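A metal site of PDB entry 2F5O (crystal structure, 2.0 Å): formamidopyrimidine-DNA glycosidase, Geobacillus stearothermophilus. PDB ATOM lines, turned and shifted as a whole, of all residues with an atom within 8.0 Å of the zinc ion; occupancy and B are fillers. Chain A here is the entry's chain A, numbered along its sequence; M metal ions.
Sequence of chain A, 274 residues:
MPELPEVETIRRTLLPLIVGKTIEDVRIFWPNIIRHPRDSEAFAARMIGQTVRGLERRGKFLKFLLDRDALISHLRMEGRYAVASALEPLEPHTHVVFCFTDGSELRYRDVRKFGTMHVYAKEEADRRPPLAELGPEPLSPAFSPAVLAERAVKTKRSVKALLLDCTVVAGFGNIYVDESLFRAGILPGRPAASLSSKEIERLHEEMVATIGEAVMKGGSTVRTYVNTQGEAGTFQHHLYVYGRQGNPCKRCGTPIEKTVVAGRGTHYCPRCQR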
ATOM      1  N   PHE A 182      -7.373  16.833 -17.684  1.00  0.00           N
ATOM      2  CA  PHE A 182      -7.775  18.253 -17.772  1.00  0.00           C
ATOM      3  C   PHE A 182      -8.605  18.456 -19.047  1.00  0.00           C
ATOM      4  O   PHE A 182      -9.694  18.987 -19.037  1.00  0.00           O
ATOM      5  CB  PHE A 182      -6.554  19.175 -17.859  1.00  0.00           C
ATOM      6  CG  PHE A 182      -6.909  20.599 -18.192  1.00  0.00           C
ATOM      7  CD1 PHE A 182      -7.368  21.461 -17.183  1.00  0.00           C
ATOM      8  CD2 PHE A 182      -6.938  21.031 -19.510  1.00  0.00           C
ATOM      9  CE1 PHE A 182      -7.869  22.781 -17.491  1.00  0.00           C
ATOM     10  CE2 PHE A 182      -7.418  22.319 -19.840  1.00  0.00           C
ATOM     11  CZ  PHE A 182      -7.892  23.190 -18.816  1.00  0.00           C
ATOM     12  N   TYR A 240      -1.377  22.593 -20.235  1.00  0.00           N
ATOM     13  CA  TYR A 240      -2.471  23.256 -19.510  1.00  0.00           C
ATOM     14  C   TYR A 240      -2.290  23.266 -18.000  1.00  0.00           C
ATOM     15  O   TYR A 240      -2.515  24.289 -17.327  1.00  0.00           O
ATOM     16  CB  TYR A 240      -3.811  22.592 -19.801  1.00  0.00           C
ATOM     17  CG  TYR A 240      -4.289  22.847 -21.184  1.00  0.00           C
ATOM     18  CD1 TYR A 240      -4.089  21.907 -22.205  1.00  0.00           C
ATOM     19  CD2 TYR A 240      -4.933  24.044 -21.489  1.00  0.00           C
ATOM     20  CE1 TYR A 240      -4.516  22.136 -23.493  1.00  0.00           C
ATOM     21  CE2 TYR A 240      -5.390  24.299 -22.791  1.00  0.00           C
ATOM     22  CZ  TYR A 240      -5.185  23.345 -23.787  1.00  0.00           C
ATOM     23  OH  TYR A 240      -5.661  23.599 -25.050  1.00  0.00           O
ATOM     24  N   VAL A 241      -1.875  22.110 -17.475  1.00  0.00           N
ATOM     25  CA  VAL A 241      -1.703  21.943 -16.041  1.00  0.00           C
ATOM     26  C   VAL A 241      -0.367  21.400 -15.520  1.00  0.00           C
ATOM     27  O   VAL A 241       0.112  21.821 -14.450  1.00  0.00           O
ATOM     28  CB  VAL A 241      -2.855  21.056 -15.477  1.00  0.00           C
ATOM     29  CG1 VAL A 241      -4.224  21.665 -15.900  1.00  0.00           C
ATOM     30  CG2 VAL A 241      -2.750  19.639 -16.024  1.00  0.00           C
ATOM     31  N   PRO A 248      -2.233  30.661 -13.351  1.00  0.00           N
ATOM     32  CA  PRO A 248      -3.647  30.607 -13.728  1.00  0.00           C
ATOM     33  C   PRO A 248      -3.894  29.540 -14.802  1.00  0.00           C
ATOM     34  O   PRO A 248      -3.017  29.294 -15.644  1.00  0.00           O
ATOM     35  CB  PRO A 248      -3.929  32.012 -14.231  1.00  0.00           C
ATOM     36  CG  PRO A 248      -2.606  32.494 -14.746  1.00  0.00           C
ATOM     37  CD  PRO A 248      -1.579  31.901 -13.812  1.00  0.00           C
ATOM     38  N   CYS A 249      -5.063  28.906 -14.739  1.00  0.00           N
ATOM     39  CA  CYS A 249      -5.472  27.922 -15.723  1.00  0.00           C
ATOM     40  C   CYS A 249      -5.624  28.714 -17.006  1.00  0.00           C
ATOM     41  O   CYS A 249      -6.148  29.844 -17.002  1.00  0.00           O
ATOM     42  CB  CYS A 249      -6.808  27.318 -15.330  1.00  0.00           C
ATOM     43  SG  CYS A 249      -7.642  26.376 -16.648  1.00  0.00           S
ATOM     44  N   LYS A 250      -5.162  28.140 -18.108  1.00  0.00           N
ATOM     45  CA  LYS A 250      -5.218  28.787 -19.414  1.00  0.00           C
ATOM     46  C   LYS A 250      -6.605  28.904 -19.981  1.00  0.00           C
ATOM     47  O   LYS A 250      -6.835  29.706 -20.891  1.00  0.00           O
ATOM     48  CB  LYS A 250      -4.304  28.041 -20.397  1.00  0.00           C
ATOM     49  CG  LYS A 250      -2.880  27.990 -19.879  1.00  0.00           C
ATOM     50  CD  LYS A 250      -1.864  27.805 -21.013  1.00  0.00           C
ATOM     51  CE  LYS A 250      -0.412  27.663 -20.455  1.00  0.00           C
ATOM     52  NZ  LYS A 250       0.654  27.551 -21.537  1.00  0.00           N
ATOM     53  N   ARG A 251      -7.530  28.126 -19.434  1.00  0.00           N
ATOM     54  CA  ARG A 251      -8.881  28.181 -19.931  1.00  0.00           C
ATOM     55  C   ARG A 251      -9.804  29.042 -19.057  1.00  0.00           C
ATOM     56  O   ARG A 251     -10.747  29.651 -19.586  1.00  0.00           O
ATOM     57  CB  ARG A 251      -9.402  26.730 -20.047  1.00  0.00           C
ATOM     58  CG  ARG A 251     -10.874  26.530 -20.127  1.00  0.00           C
ATOM     59  CD  ARG A 251     -11.174  25.414 -21.104  1.00  0.00           C
ATOM     60  NE  ARG A 251     -11.319  24.099 -20.491  1.00  0.00           N
ATOM     61  CZ  ARG A 251     -10.908  22.962 -21.055  1.00  0.00           C
ATOM     62  NH1 ARG A 251     -11.099  21.792 -20.426  1.00  0.00           N
ATOM     63  NH2 ARG A 251     -10.265  22.978 -22.228  1.00  0.00           N
ATOM     64  N   CYS A 252      -9.566  29.118 -17.736  1.00  0.00           N
ATOM     65  CA  CYS A 252     -10.467  29.887 -16.887  1.00  0.00           C
ATOM     66  C   CYS A 252      -9.793  30.816 -15.910  1.00  0.00           C
ATOM     67  O   CYS A 252     -10.462  31.535 -15.194  1.00  0.00           O
ATOM     68  CB  CYS A 252     -11.395  28.945 -16.074  1.00  0.00           C
ATOM     69  SG  CYS A 252     -10.545  28.103 -14.671  1.00  0.00           S
ATOM     70  N   GLY A 253      -8.469  30.774 -15.819  1.00  0.00           N
ATOM     71  CA  GLY A 253      -7.793  31.673 -14.921  1.00  0.00           C
ATOM     72  C   GLY A 253      -7.694  31.228 -13.489  1.00  0.00           C
ATOM     73  O   GLY A 253      -6.993  31.866 -12.710  1.00  0.00           O
ATOM     74  N   THR A 254      -8.400  30.167 -13.093  1.00  0.00           N
ATOM     75  CA  THR A 254      -8.327  29.661 -11.733  1.00  0.00           C
ATOM     76  C   THR A 254      -6.901  29.087 -11.500  1.00  0.00           C
ATOM     77  O   THR A 254      -6.313  28.434 -12.388  1.00  0.00           O
ATOM     78  CB  THR A 254      -9.346  28.531 -11.549  1.00  0.00           C
ATOM     79  OG1 THR A 254     -10.665  29.075 -11.636  1.00  0.00           O
ATOM     80  CG2 THR A 254      -9.147  27.822 -10.224  1.00  0.00           C
ATOM     81  N   PRO A 255      -6.293  29.330 -10.329  1.00  0.00           N
ATOM     82  CA  PRO A 255      -4.951  28.762 -10.114  1.00  0.00           C
ATOM     83  C   PRO A 255      -4.909  27.224 -10.178  1.00  0.00           C
ATOM     84  O   PRO A 255      -5.699  26.509  -9.545  1.00  0.00           O
ATOM     85  CB  PRO A 255      -4.595  29.268  -8.714  1.00  0.00           C
ATOM     86  CG  PRO A 255      -5.278  30.600  -8.653  1.00  0.00           C
ATOM     87  CD  PRO A 255      -6.647  30.264  -9.234  1.00  0.00           C
ATOM     88  N   ILE A 256      -3.945  26.710 -10.928  1.00  0.00           N
ATOM     89  CA  ILE A 256      -3.786  25.266 -11.039  1.00  0.00           C
ATOM     90  C   ILE A 256      -3.308  24.702  -9.688  1.00  0.00           C
ATOM     91  O   ILE A 256      -2.440  25.278  -9.042  1.00  0.00           O
ATOM     92  CB  ILE A 256      -2.757  24.963 -12.125  1.00  0.00           C
ATOM     93  CG1 ILE A 256      -3.380  25.361 -13.478  1.00  0.00           C
ATOM     94  CG2 ILE A 256      -2.305  23.480 -12.095  1.00  0.00           C
ATOM     95  CD1 ILE A 256      -4.835  24.758 -13.602  1.00  0.00           C
ATOM     96  N   TYR A 268      -4.031  19.824 -11.580  1.00  0.00           N
ATOM     97  CA  TYR A 268      -5.388  19.891 -12.127  1.00  0.00           C
ATOM     98  C   TYR A 268      -6.018  21.272 -11.864  1.00  0.00           C
ATOM     99  O   TYR A 268      -5.530  22.030 -11.034  1.00  0.00           O
ATOM    100  CB  TYR A 268      -6.270  18.783 -11.497  1.00  0.00           C
ATOM    101  CG  TYR A 268      -6.428  18.904  -9.998  1.00  0.00           C
ATOM    102  CD1 TYR A 268      -7.409  19.726  -9.454  1.00  0.00           C
ATOM    103  CD2 TYR A 268      -5.496  18.322  -9.126  1.00  0.00           C
ATOM    104  CE1 TYR A 268      -7.460  19.977  -8.126  1.00  0.00           C
ATOM    105  CE2 TYR A 268      -5.542  18.564  -7.764  1.00  0.00           C
ATOM    106  CZ  TYR A 268      -6.534  19.408  -7.279  1.00  0.00           C
ATOM    107  OH  TYR A 268      -6.594  19.745  -5.959  1.00  0.00           O
ATOM    108  N   CYS A 269      -7.066  21.580 -12.618  1.00  0.00           N
ATOM    109  CA  CYS A 269      -7.824  22.842 -12.432  1.00  0.00           C
ATOM    110  C   CYS A 269      -9.042  22.434 -11.608  1.00  0.00           C
ATOM    111  O   CYS A 269      -9.846  21.623 -12.037  1.00  0.00           O
ATOM    112  CB  CYS A 269      -8.285  23.429 -13.774  1.00  0.00           C
ATOM    113  SG  CYS A 269      -9.461  24.816 -13.519  1.00  0.00           S
ATOM    114  N   PRO A 270      -9.194  22.977 -10.394  1.00  0.00           N
ATOM    115  CA  PRO A 270     -10.333  22.633  -9.559  1.00  0.00           C
ATOM    116  C   PRO A 270     -11.680  23.053 -10.084  1.00  0.00           C
ATOM    117  O   PRO A 270     -12.709  22.462  -9.760  1.00  0.00           O
ATOM    118  CB  PRO A 270     -10.022  23.290  -8.213  1.00  0.00           C
ATOM    119  CG  PRO A 270      -9.082  24.350  -8.534  1.00  0.00           C
ATOM    120  CD  PRO A 270      -8.232  23.825  -9.672  1.00  0.00           C
ATOM    121  N   ARG A 271     -11.700  24.076 -10.911  1.00  0.00           N
ATOM    122  CA  ARG A 271     -12.964  24.557 -11.486  1.00  0.00           C
ATOM    123  C   ARG A 271     -13.402  23.728 -12.682  1.00  0.00           C
ATOM    124  O   ARG A 271     -14.557  23.307 -12.767  1.00  0.00           O
ATOM    125  CB  ARG A 271     -12.811  26.020 -11.946  1.00  0.00           C
ATOM    126  CG  ARG A 271     -14.064  26.576 -12.583  1.00  0.00           C
ATOM    127  CD  ARG A 271     -13.877  27.982 -13.108  1.00  0.00           C
ATOM    128  NE  ARG A 271     -15.137  28.407 -13.715  1.00  0.00           N
ATOM    129  CZ  ARG A 271     -15.460  29.670 -14.001  1.00  0.00           C
ATOM    130  NH1 ARG A 271     -16.660  29.896 -14.526  1.00  0.00           N
ATOM    131  NH2 ARG A 271     -14.622  30.682 -13.774  1.00  0.00           N
ATOM    132  N   CYS A 272     -12.485  23.479 -13.608  1.00  0.00           N
ATOM    133  CA  CYS A 272     -12.835  22.756 -14.826  1.00  0.00           C
ATOM    134  C   CYS A 272     -12.874  21.216 -14.796  1.00  0.00           C
ATOM    135  O   CYS A 272     -13.449  20.605 -15.670  1.00  0.00           O
ATOM    136  CB  CYS A 272     -11.916  23.213 -15.945  1.00  0.00           C
ATOM    137  SG  CYS A 272     -12.043  25.063 -16.310  1.00  0.00           S
ATOM    138  N   GLN A 273     -12.221  20.601 -13.834  1.00  0.00           N
ATOM    139  CA  GLN A 273     -12.270  19.163 -13.772  1.00  0.00           C
ATOM    140  C   GLN A 273     -13.191  18.834 -12.617  1.00  0.00           C
ATOM    141  O   GLN A 273     -13.113  19.456 -11.577  1.00  0.00           O
ATOM    142  CB  GLN A 273     -10.851  18.588 -13.527  1.00  0.00           C
ATOM    143  CG  GLN A 273      -9.959  18.765 -14.744  1.00  0.00           C
ATOM    144  CD  GLN A 273      -8.533  18.479 -14.450  1.00  0.00           C
ATOM    145  OE1 GLN A 273      -7.734  19.369 -14.414  1.00  0.00           O
ATOM    146  NE2 GLN A 273      -8.208  17.216 -14.242  1.00  0.00           N
HETATM  147 ZN    ZN M   1      -9.637  26.037 -15.463  1.00  0.00          ZN
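The backbone NH (N) of Cys 249 lies within hydrogen-bond range of the backbone carbonyl oxygen (O) of Thr 254 (2.7 Å).
The backbone NH (N) of Cys 269 lies within hydrogen-bond range of the side-chain amide oxygen (OE1) of Gln 273, 2.9 Å away.
OG1 of Thr 254 lies close to SG of Cys 252.
The side-chain sulfur of Cys 249 lies close to the backbone NH of Arg 251 (3.3 Å).
The backbone NH of Arg 271 lies close to the side-chain sulfur of Cys 269 (3.5 Å).
The zinc ion is bound by SG of Cys 269 (2.3 Å).
The side-chain sulfur (SG) of Cys 249 is bound to the zinc ion.
The zinc ion is bound by the side-chain sulfur (SG) of Cys 252 (2.4 Å).
The zinc ion is bound by SG of Cys 272.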
